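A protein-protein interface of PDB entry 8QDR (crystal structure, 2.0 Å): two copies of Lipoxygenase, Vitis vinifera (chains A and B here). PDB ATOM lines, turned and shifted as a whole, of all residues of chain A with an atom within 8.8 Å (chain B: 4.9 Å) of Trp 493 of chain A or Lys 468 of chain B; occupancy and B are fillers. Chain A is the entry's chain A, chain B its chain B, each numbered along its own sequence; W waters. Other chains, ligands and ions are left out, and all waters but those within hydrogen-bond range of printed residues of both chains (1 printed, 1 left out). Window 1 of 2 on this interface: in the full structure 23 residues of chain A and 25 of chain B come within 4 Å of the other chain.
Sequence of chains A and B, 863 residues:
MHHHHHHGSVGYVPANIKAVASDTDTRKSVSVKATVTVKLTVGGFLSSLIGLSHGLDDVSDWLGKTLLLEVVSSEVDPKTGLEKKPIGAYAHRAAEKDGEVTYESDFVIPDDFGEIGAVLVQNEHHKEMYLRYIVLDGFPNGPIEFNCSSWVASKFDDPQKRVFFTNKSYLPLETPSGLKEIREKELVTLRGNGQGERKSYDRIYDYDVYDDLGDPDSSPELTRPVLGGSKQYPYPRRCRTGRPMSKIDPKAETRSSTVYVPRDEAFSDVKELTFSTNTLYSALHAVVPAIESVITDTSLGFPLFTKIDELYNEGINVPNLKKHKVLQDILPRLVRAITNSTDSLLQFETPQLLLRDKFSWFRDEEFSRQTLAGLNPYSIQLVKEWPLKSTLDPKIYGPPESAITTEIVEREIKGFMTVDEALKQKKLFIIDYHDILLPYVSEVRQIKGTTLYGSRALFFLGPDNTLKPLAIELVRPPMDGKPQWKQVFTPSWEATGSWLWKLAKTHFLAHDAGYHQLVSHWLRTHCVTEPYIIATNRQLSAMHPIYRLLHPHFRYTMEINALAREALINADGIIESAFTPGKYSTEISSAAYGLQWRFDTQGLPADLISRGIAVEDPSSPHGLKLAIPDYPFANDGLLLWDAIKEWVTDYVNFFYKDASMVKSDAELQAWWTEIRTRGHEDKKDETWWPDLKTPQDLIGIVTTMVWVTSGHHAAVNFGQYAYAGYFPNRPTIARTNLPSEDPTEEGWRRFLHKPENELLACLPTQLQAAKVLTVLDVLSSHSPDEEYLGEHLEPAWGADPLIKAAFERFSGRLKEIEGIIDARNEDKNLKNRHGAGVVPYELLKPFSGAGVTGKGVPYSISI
The backbone carbonyl oxygen (O) of Trp 493 of chain A is in hydrogen-bond range of the side-chain hydroxyl (OG1) of Thr 466 of chain B, 3.1 Å away.
Printed residues of chain B within 4 Å of Arg 411 of chain A: Phe 416 (3.6 Å). Glu 412 of chain A touches none of the printed residues of chain B. Trp 493 of chain A touches just these residues of chain B: Glu 365 (3.6 Å), Phe 416 (3.2 Å), Phe 460 (3.8 Å), Pro 463 (3.9 Å), Thr 466 (3.1 Å) and Lys 468 (3.5 Å). Of the printed residues of chain B, Ala 495 of chain A touches Glu 365. Of the printed residues of chain A, Phe 416 of chain B touches Arg 411 (3.6 Å) and Trp 493 (3.2 Å). Leu 467 of chain B touches none of the printed residues of chain A. Lys 468 of chain B touches just one residue of chain A: Trp 493 (3.5 Å). The nearest residue of chain A that does not touch Lys 468 of chain B is Ser 492 of chain A (6.9 Å).
Of the 15 printed residues of chain B, 6 touch a printed residue of chain A. Printed residues of chain B that touch a printed residue of chain A: Glu 365, Phe 416, Phe 460, Pro 463, Thr 466 and Lys 468. Along chain B the printed residues that touch a printed residue of chain A span positions 365 to 468. Hydrophobic or aromatic side chains of chain A that line the printed part of chain B: Trp 493.
Water W1 bridges O of Glu 412 of chain B (2.9 Å) and O of Arg 411 of chain A (2.9 Å).
Arg 411 of chain A touches Phe 416 of chain B (CD to CE1, 3.6 Å). Glu 365 of chain B touches Trp 493 of chain A. CH2 of Trp 493 of chain A touches CE2 of Phe 416 of chain B, 3.2 Å away. Trp 493 of chain A touches Phe 460 of chain B. CZ3 of Trp 493 of chain A touches CD of Pro 463 of chain B, 3.9 Å away. Trp 493 of chain A touches Lys 468 of chain B. C of Glu 494 of chain A touches CG of Glu 365 of chain B, 3.9 Å away. Glu 494 of chain A touches Thr 466 of chain B (CB to CG2, 3.98 Å). Glu 365 of chain B touches Ala 495 of chain A. Ser 498 of chain A touches Glu 365 of chain B.
The side-chain carboxylate (OE1) of Glu 494 of chain A lies within hydrogen-bond range of the backbone NH (N) of Thr 496 of chain A. The backbone NH (N) of Glu 494 of chain A is in hydrogen-bond range of the side-chain hydroxyl (OG) of Ser 492 of chain A, at 3.2 Å. The backbone NH (N) of Lys 468 of chain B lies within hydrogen-bond range of the backbone carbonyl oxygen (O) of Phe 460 of chain B. OE2 of Glu 494 of chain A sits at hydrogen-bond distance from N of Gly 497 of chain A. The side-chain carboxylate (OE1) of Glu 412 of chain B is in salt-bridge range of the side-chain amino group (NZ) of Lys 468 of chain B (2.9 Å).
Positions printed for both chains: 412, 468 and 491.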
ATOM      1  N   ARG A 411      17.484   6.255  10.276  1.00  0.00           N
ATOM      2  CA  ARG A 411      18.266   7.370  10.807  1.00  0.00           C
ATOM      3  C   ARG A 411      19.508   7.638   9.967  1.00  0.00           C
ATOM      4  O   ARG A 411      20.010   8.770   9.945  1.00  0.00           O
ATOM      5  CB  ARG A 411      18.697   7.105  12.249  1.00  0.00           C
ATOM      6  CG  ARG A 411      17.571   6.946  13.220  1.00  0.00           C
ATOM      7  CD  ARG A 411      16.798   8.232  13.391  1.00  0.00           C
ATOM      8  NE  ARG A 411      15.900   8.151  14.549  1.00  0.00           N
ATOM      9  CZ  ARG A 411      14.971   9.052  14.834  1.00  0.00           C
ATOM     10  NH1 ARG A 411      14.804  10.114  14.052  1.00  0.00           N
ATOM     11  NH2 ARG A 411      14.209   8.889  15.905  1.00  0.00           N
ATOM     12  N   GLU A 412      20.036   6.621   9.295  1.00  0.00           N
ATOM     13  CA  GLU A 412      21.294   6.780   8.578  1.00  0.00           C
ATOM     14  C   GLU A 412      21.124   7.072   7.103  1.00  0.00           C
ATOM     15  O   GLU A 412      21.993   7.729   6.524  1.00  0.00           O
ATOM     16  CB  GLU A 412      22.157   5.528   8.722  1.00  0.00           C
ATOM     17  CG  GLU A 412      22.247   5.041  10.137  1.00  0.00           C
ATOM     18  CD  GLU A 412      23.321   3.993  10.307  1.00  0.00           C
ATOM     19  OE1 GLU A 412      24.420   4.156   9.738  1.00  0.00           O
ATOM     20  OE2 GLU A 412      23.061   3.002  11.008  1.00  0.00           O
ATOM     21  N   LYS A 468      28.224   1.959   2.513  1.00  0.00           N
ATOM     22  CA  LYS A 468      28.305   2.621   3.798  1.00  0.00           C
ATOM     23  C   LYS A 468      27.914   1.609   4.859  1.00  0.00           C
ATOM     24  O   LYS A 468      26.819   1.030   4.775  1.00  0.00           O
ATOM     25  CB  LYS A 468      27.385   3.836   3.851  1.00  0.00           C
ATOM     26  CG  LYS A 468      27.437   4.585   5.200  1.00  0.00           C
ATOM     27  CD  LYS A 468      26.100   5.237   5.575  1.00  0.00           C
ATOM     28  CE  LYS A 468      26.211   6.095   6.864  1.00  0.00           C
ATOM     29  NZ  LYS A 468      26.883   5.356   7.992  1.00  0.00           N
ATOM     30  N   THR A 490      26.262   0.911  15.779  1.00  0.00           N
ATOM     31  CA  THR A 490      26.304   1.677  14.542  1.00  0.00           C
ATOM     32  C   THR A 490      27.407   2.720  14.642  1.00  0.00           C
ATOM     33  O   THR A 490      27.851   3.054  15.747  1.00  0.00           O
ATOM     34  CB  THR A 490      24.976   2.394  14.267  1.00  0.00           C
ATOM     35  OG1 THR A 490      24.846   3.472  15.197  1.00  0.00           O
ATOM     36  CG2 THR A 490      23.784   1.447  14.416  1.00  0.00           C
ATOM     37  N   PRO A 491      27.866   3.265  13.505  1.00  0.00           N
ATOM     38  CA  PRO A 491      28.716   4.462  13.571  1.00  0.00           C
ATOM     39  C   PRO A 491      27.990   5.533  14.387  1.00  0.00           C
ATOM     40  O   PRO A 491      26.766   5.645  14.329  1.00  0.00           O
ATOM     41  CB  PRO A 491      28.889   4.869  12.100  1.00  0.00           C
ATOM     42  CG  PRO A 491      28.665   3.569  11.301  1.00  0.00           C
ATOM     43  CD  PRO A 491      27.651   2.790  12.123  1.00  0.00           C
ATOM     44  N   SER A 492      28.734   6.292  15.188  1.00  0.00           N
ATOM     45  CA  SER A 492      28.096   7.113  16.215  1.00  0.00           C
ATOM     46  C   SER A 492      28.660   8.527  16.245  1.00  0.00           C
ATOM     47  O   SER A 492      29.795   8.775  15.851  1.00  0.00           O
ATOM     48  CB  SER A 492      28.243   6.493  17.604  1.00  0.00           C
ATOM     49  OG  SER A 492      27.710   7.370  18.585  1.00  0.00           O
ATOM     50  N   TRP A 493      27.848   9.458  16.742  1.00  0.00           N
ATOM     51  CA  TRP A 493      28.253  10.857  16.846  1.00  0.00           C
ATOM     52  C   TRP A 493      28.745  11.235  18.246  1.00  0.00           C
ATOM     53  O   TRP A 493      28.963  12.420  18.512  1.00  0.00           O
ATOM     54  CB  TRP A 493      27.094  11.769  16.431  1.00  0.00           C
ATOM     55  CG  TRP A 493      26.592  11.533  15.028  1.00  0.00           C
ATOM     56  CD1 TRP A 493      27.203  10.820  14.040  1.00  0.00           C
ATOM     57  CD2 TRP A 493      25.365  12.024  14.471  1.00  0.00           C
ATOM     58  NE1 TRP A 493      26.432  10.844  12.893  1.00  0.00           N
ATOM     59  CE2 TRP A 493      25.305  11.588  13.134  1.00  0.00           C
ATOM     60  CE3 TRP A 493      24.330  12.821  14.969  1.00  0.00           C
ATOM     61  CZ2 TRP A 493      24.235  11.903  12.294  1.00  0.00           C
ATOM     62  CZ3 TRP A 493      23.279  13.140  14.137  1.00  0.00           C
ATOM     63  CH2 TRP A 493      23.237  12.681  12.812  1.00  0.00           C
ATOM     64  N   GLU A 494      28.929  10.264  19.141  1.00  0.00           N
ATOM     65  CA  GLU A 494      29.424  10.532  20.490  1.00  0.00           C
ATOM     66  C   GLU A 494      30.444   9.458  20.874  1.00  0.00           C
ATOM     67  O   GLU A 494      30.475   8.371  20.292  1.00  0.00           O
ATOM     68  CB  GLU A 494      28.258  10.601  21.483  1.00  0.00           C
ATOM     69  CG  GLU A 494      27.415   9.337  21.488  1.00  0.00           C
ATOM     70  CD  GLU A 494      27.791   8.405  22.630  1.00  0.00           C
ATOM     71  OE1 GLU A 494      28.381   8.892  23.616  1.00  0.00           O
ATOM     72  OE2 GLU A 494      27.495   7.198  22.542  1.00  0.00           O
ATOM     73  N   ALA A 495      31.285   9.764  21.872  1.00  0.00           N
ATOM     74  CA  ALA A 495      32.500   8.969  22.094  1.00  0.00           C
ATOM     75  C   ALA A 495      32.195   7.511  22.461  1.00  0.00           C
ATOM     76  O   ALA A 495      32.805   6.588  21.910  1.00  0.00           O
ATOM     77  CB  ALA A 495      33.359   9.616  23.177  1.00  0.00           C
ATOM     78  N   THR A 496      31.283   7.284  23.416  1.00  0.00           N
ATOM     79  CA  THR A 496      31.027   5.930  23.901  1.00  0.00           C
ATOM     80  C   THR A 496      30.463   5.042  22.803  1.00  0.00           C
ATOM     81  O   THR A 496      30.888   3.893  22.645  1.00  0.00           O
ATOM     82  CB  THR A 496      30.072   5.958  25.090  1.00  0.00           C
ATOM     83  OG1 THR A 496      30.693   6.648  26.175  1.00  0.00           O
ATOM     84  CG2 THR A 496      29.721   4.549  25.529  1.00  0.00           C
ATOM     85  N   GLY A 497      29.490   5.560  22.040  1.00  0.00           N
ATOM     86  CA  GLY A 497      28.921   4.787  20.952  1.00  0.00           C
ATOM     87  C   GLY A 497      29.917   4.541  19.843  1.00  0.00           C
ATOM     88  O   GLY A 497      29.857   3.515  19.164  1.00  0.00           O
ATOM     89  N   SER A 498      30.860   5.464  19.664  1.00  0.00           N
ATOM     90  CA  SER A 498      31.892   5.294  18.653  1.00  0.00           C
ATOM     91  C   SER A 498      32.891   4.214  19.067  1.00  0.00           C
ATOM     92  O   SER A 498      33.283   3.368  18.249  1.00  0.00           O
ATOM     93  CB  SER A 498      32.582   6.640  18.414  1.00  0.00           C
ATOM     94  OG  SER A 498      33.529   6.576  17.366  1.00  0.00           O
ATOM     95  N   TRP A 499      33.311   4.221  20.329  1.00  0.00           N
ATOM     96  CA  TRP A 499      34.194   3.166  20.818  1.00  0.00           C
ATOM     97  C   TRP A 499      33.509   1.806  20.795  1.00  0.00           C
ATOM     98  O   TRP A 499      34.137   0.793  20.478  1.00  0.00           O
ATOM     99  CB  TRP A 499      34.660   3.484  22.235  1.00  0.00           C
ATOM    100  CG  TRP A 499      36.005   4.107  22.286  1.00  0.00           C
ATOM    101  CD1 TRP A 499      36.296   5.397  22.581  1.00  0.00           C
ATOM    102  CD2 TRP A 499      37.251   3.462  22.016  1.00  0.00           C
ATOM    103  NE1 TRP A 499      37.651   5.602  22.521  1.00  0.00           N
ATOM    104  CE2 TRP A 499      38.263   4.429  22.174  1.00  0.00           C
ATOM    105  CE3 TRP A 499      37.612   2.158  21.652  1.00  0.00           C
ATOM    106  CZ2 TRP A 499      39.614   4.140  21.991  1.00  0.00           C
ATOM    107  CZ3 TRP A 499      38.959   1.870  21.471  1.00  0.00           C
ATOM    108  CH2 TRP A 499      39.943   2.860  21.641  1.00  0.00           C
ATOM    109  N   TRP A 501      31.300   0.908  18.680  1.00  0.00           N
ATOM    110  CA  TRP A 501      31.304   0.535  17.261  1.00  0.00           C
ATOM    111  C   TRP A 501      32.642  -0.072  16.851  1.00  0.00           C
ATOM    112  O   TRP A 501      32.679  -1.065  16.117  1.00  0.00           O
ATOM    113  CB  TRP A 501      30.966   1.761  16.402  1.00  0.00           C
ATOM    114  CG  TRP A 501      31.188   1.591  14.900  1.00  0.00           C
ATOM    115  CD1 TRP A 501      32.108   2.245  14.125  1.00  0.00           C
ATOM    116  CD2 TRP A 501      30.464   0.730  14.015  1.00  0.00           C
ATOM    117  NE1 TRP A 501      32.007   1.833  12.819  1.00  0.00           N
ATOM    118  CE2 TRP A 501      31.007   0.905  12.721  1.00  0.00           C
ATOM    119  CE3 TRP A 501      29.415  -0.178  14.187  1.00  0.00           C
ATOM    120  CZ2 TRP A 501      30.541   0.200  11.617  1.00  0.00           C
ATOM    121  CZ3 TRP A 501      28.949  -0.865  13.104  1.00  0.00           C
ATOM    122  CH2 TRP A 501      29.512  -0.678  11.821  1.00  0.00           C
ATOM    123  N   GLU B 365      33.878  13.114  16.265  1.00  0.00           N
ATOM    124  CA  GLU B 365      33.164  13.510  17.468  1.00  0.00           C
ATOM    125  C   GLU B 365      34.066  14.255  18.456  1.00  0.00           C
ATOM    126  O   GLU B 365      33.558  15.051  19.250  1.00  0.00           O
ATOM    127  CB  GLU B 365      32.488  12.280  18.096  1.00  0.00           C
ATOM    128  CG  GLU B 365      33.244  11.593  19.212  1.00  0.00           C
ATOM    129  CD  GLU B 365      34.367  10.687  18.744  1.00  0.00           C
ATOM    130  OE1 GLU B 365      35.395  10.613  19.465  1.00  0.00           O
ATOM    131  OE2 GLU B 365      34.219  10.046  17.681  1.00  0.00           O
ATOM    132  N   SER B 368      34.452  17.841  17.073  1.00  0.00           N
ATOM    133  CA  SER B 368      33.241  18.608  17.361  1.00  0.00           C
ATOM    134  C   SER B 368      33.147  18.958  18.833  1.00  0.00           C
ATOM    135  O   SER B 368      32.815  20.096  19.194  1.00  0.00           O
ATOM    136  CB  SER B 368      32.011  17.814  16.931  1.00  0.00           C
ATOM    137  OG  SER B 368      32.069  17.664  15.537  1.00  0.00           O
ATOM    138  N   GLU B 412      22.844  14.232   5.128  1.00  0.00           N
ATOM    139  CA  GLU B 412      23.422  13.820   6.401  1.00  0.00           C
ATOM    140  C   GLU B 412      22.417  13.737   7.557  1.00  0.00           C
ATOM    141  O   GLU B 412      22.557  12.857   8.412  1.00  0.00           O
ATOM    142  CB  GLU B 412      24.556  14.776   6.790  1.00  0.00           C
ATOM    143  CG  GLU B 412      25.753  14.699   5.877  1.00  0.00           C
ATOM    144  CD  GLU B 412      26.883  15.597   6.331  1.00  0.00           C
ATOM    145  OE1 GLU B 412      27.418  15.349   7.431  1.00  0.00           O
ATOM    146  OE2 GLU B 412      27.232  16.547   5.591  1.00  0.00           O
ATOM    147  N   PHE B 416      16.890  12.503  10.989  1.00  0.00           N
ATOM    148  CA  PHE B 416      16.439  13.187  12.194  1.00  0.00           C
ATOM    149  C   PHE B 416      15.531  14.369  11.909  1.00  0.00           C
ATOM    150  O   PHE B 416      14.507  14.519  12.580  1.00  0.00           O
ATOM    151  CB  PHE B 416      17.649  13.651  13.004  1.00  0.00           C
ATOM    152  CG  PHE B 416      18.492  12.517  13.508  1.00  0.00           C
ATOM    153  CD1 PHE B 416      18.070  11.753  14.588  1.00  0.00           C
ATOM    154  CD2 PHE B 416      19.683  12.191  12.896  1.00  0.00           C
ATOM    155  CE1 PHE B 416      18.829  10.700  15.056  1.00  0.00           C
ATOM    156  CE2 PHE B 416      20.446  11.129  13.364  1.00  0.00           C
ATOM    157  CZ  PHE B 416      20.019  10.389  14.446  1.00  0.00           C
ATOM    158  N   LEU B 458      30.513  23.727   9.717  1.00  0.00           N
ATOM    159  CA  LEU B 458      29.097  23.630  10.066  1.00  0.00           C
ATOM    160  C   LEU B 458      28.837  22.382  10.906  1.00  0.00           C
ATOM    161  O   LEU B 458      29.410  21.320  10.641  1.00  0.00           O
ATOM    162  CB  LEU B 458      28.238  23.607   8.801  1.00  0.00           C
ATOM    163  CG  LEU B 458      26.716  23.646   8.939  1.00  0.00           C
ATOM    164  CD1 LEU B 458      26.238  24.977   9.502  1.00  0.00           C
ATOM    165  CD2 LEU B 458      26.057  23.339   7.576  1.00  0.00           C
ATOM    166  N   PHE B 459      27.971  22.513  11.922  1.00  0.00           N
ATOM    167  CA  PHE B 459      27.685  21.428  12.860  1.00  0.00           C
ATOM    168  C   PHE B 459      26.189  21.270  13.094  1.00  0.00           C
ATOM    169  O   PHE B 459      25.448  22.257  13.160  1.00  0.00           O
ATOM    170  CB  PHE B 459      28.349  21.652  14.220  1.00  0.00           C
ATOM    171  CG  PHE B 459      29.824  21.859  14.135  1.00  0.00           C
ATOM    172  CD1 PHE B 459      30.339  23.129  13.893  1.00  0.00           C
ATOM    173  CD2 PHE B 459      30.692  20.785  14.274  1.00  0.00           C
ATOM    174  CE1 PHE B 459      31.705  23.332  13.823  1.00  0.00           C
ATOM    175  CE2 PHE B 459      32.068  20.965  14.197  1.00  0.00           C
ATOM    176  CZ  PHE B 459      32.575  22.237  13.956  1.00  0.00           C
ATOM    177  N   PHE B 460      25.768  20.011  13.250  1.00  0.00           N
ATOM    178  CA  PHE B 460      24.410  19.643  13.624  1.00  0.00           C
ATOM    179  C   PHE B 460      24.414  19.208  15.088  1.00  0.00           C
ATOM    180  O   PHE B 460      25.247  18.389  15.486  1.00  0.00           O
ATOM    181  CB  PHE B 460      23.893  18.509  12.711  1.00  0.00           C
ATOM    182  CG  PHE B 460      22.503  18.027  13.055  1.00  0.00           C
ATOM    183  CD1 PHE B 460      21.416  18.888  12.984  1.00  0.00           C
ATOM    184  CD2 PHE B 460      22.281  16.719  13.438  1.00  0.00           C
ATOM    185  CE1 PHE B 460      20.143  18.452  13.302  1.00  0.00           C
ATOM    186  CE2 PHE B 460      20.999  16.282  13.761  1.00  0.00           C
ATOM    187  CZ  PHE B 460      19.934  17.147  13.684  1.00  0.00           C
ATOM    188  N   GLY B 462      22.925  16.913  17.524  1.00  0.00           N
ATOM    189  CA  GLY B 462      22.172  15.687  17.333  1.00  0.00           C
ATOM    190  C   GLY B 462      21.429  15.168  18.558  1.00  0.00           C
ATOM    191  O   GLY B 462      21.265  15.862  19.573  1.00  0.00           O
ATOM    192  N   PRO B 463      20.982  13.908  18.480  1.00  0.00           N
ATOM    193  CA  PRO B 463      20.041  13.386  19.490  1.00  0.00           C
ATOM    194  C   PRO B 463      20.654  13.140  20.855  1.00  0.00           C
ATOM    195  O   PRO B 463      19.902  12.955  21.816  1.00  0.00           O
ATOM    196  CB  PRO B 463      19.546  12.069  18.864  1.00  0.00           C
ATOM    197  CG  PRO B 463      20.651  11.658  17.952  1.00  0.00           C
ATOM    198  CD  PRO B 463      21.242  12.929  17.406  1.00  0.00           C
ATOM    199  N   THR B 466      25.110  16.148  21.277  1.00  0.00           N
ATOM    200  CA  THR B 466      26.485  16.290  20.831  1.00  0.00           C
ATOM    201  C   THR B 466      26.473  16.815  19.405  1.00  0.00           C
ATOM    202  O   THR B 466      25.533  16.561  18.650  1.00  0.00           O
ATOM    203  CB  THR B 466      27.268  14.967  20.869  1.00  0.00           C
ATOM    204  OG1 THR B 466      26.706  14.024  19.937  1.00  0.00           O
ATOM    205  CG2 THR B 466      27.260  14.376  22.263  1.00  0.00           C
ATOM    206  N   LEU B 467      27.538  17.523  19.044  1.00  0.00           N
ATOM    207  CA  LEU B 467      27.652  18.106  17.715  1.00  0.00           C
ATOM    208  C   LEU B 467      28.221  17.114  16.718  1.00  0.00           C
ATOM    209  O   LEU B 467      29.194  16.410  17.008  1.00  0.00           O
ATOM    210  CB  LEU B 467      28.542  19.347  17.750  1.00  0.00           C
ATOM    211  CG  LEU B 467      27.981  20.492  18.567  1.00  0.00           C
ATOM    212  CD1 LEU B 467      29.061  21.572  18.700  1.00  0.00           C
ATOM    213  CD2 LEU B 467      26.741  21.011  17.874  1.00  0.00           C
ATOM    214  N   LYS B 468      27.621  17.079  15.534  1.00  0.00           N
ATOM    215  CA  LYS B 468      28.092  16.258  14.431  1.00  0.00           C
ATOM    216  C   LYS B 468      28.643  17.181  13.351  1.00  0.00           C
ATOM    217  O   LYS B 468      27.925  18.091  12.910  1.00  0.00           O
ATOM    218  CB  LYS B 468      26.959  15.390  13.889  1.00  0.00           C
ATOM    219  CG  LYS B 468      27.356  14.447  12.736  1.00  0.00           C
ATOM    220  CD  LYS B 468      26.412  14.574  11.536  1.00  0.00           C
ATOM    221  CE  LYS B 468      26.738  13.571  10.397  1.00  0.00           C
ATOM    222  NZ  LYS B 468      28.099  13.807   9.795  1.00  0.00           N
ATOM    223  N   PRO B 469      29.890  17.017  12.909  1.00  0.00           N
ATOM    224  CA  PRO B 469      30.398  17.877  11.827  1.00  0.00           C
ATOM    225  C   PRO B 469      29.662  17.577  10.528  1.00  0.00           C
ATOM    226  O   PRO B 469      29.539  16.421  10.126  1.00  0.00           O
ATOM    227  CB  PRO B 469      31.887  17.511  11.724  1.00  0.00           C
ATOM    228  CG  PRO B 469      32.151  16.459  12.767  1.00  0.00           C
ATOM    229  CD  PRO B 469      30.828  15.941  13.265  1.00  0.00           C
ATOM    230  N   LEU B 470      29.150  18.622   9.885  1.00  0.00           N
ATOM    231  CA  LEU B 470      28.473  18.476   8.603  1.00  0.00           C
ATOM    232  C   LEU B 470      29.364  18.806   7.412  1.00  0.00           C
ATOM    233  O   LEU B 470      29.304  18.118   6.385  1.00  0.00           O
ATOM    234  CB  LEU B 470      27.241  19.377   8.549  1.00  0.00           C
ATOM    235  CG  LEU B 470      26.112  19.032   9.518  1.00  0.00           C
ATOM    236  CD1 LEU B 470      25.064  20.114   9.421  1.00  0.00           C
ATOM    237  CD2 LEU B 470      25.527  17.653   9.174  1.00  0.00           C
ATOM    238  N   PRO B 491      32.328  14.711   5.971  1.00  0.00           N
ATOM    239  CA  PRO B 491      32.635  13.314   6.327  1.00  0.00           C
ATOM    240  C   PRO B 491      32.180  12.370   5.222  1.00  0.00           C
ATOM    241  O   PRO B 491      31.167  12.608   4.561  1.00  0.00           O
ATOM    242  CB  PRO B 491      31.846  13.094   7.625  1.00  0.00           C
ATOM    243  CG  PRO B 491      31.835  14.446   8.257  1.00  0.00           C
ATOM    244  CD  PRO B 491      31.710  15.432   7.099  1.00  0.00           C
HETATM  245  O   HOH W   1      20.182  11.179   8.266  1.00  0.00           O
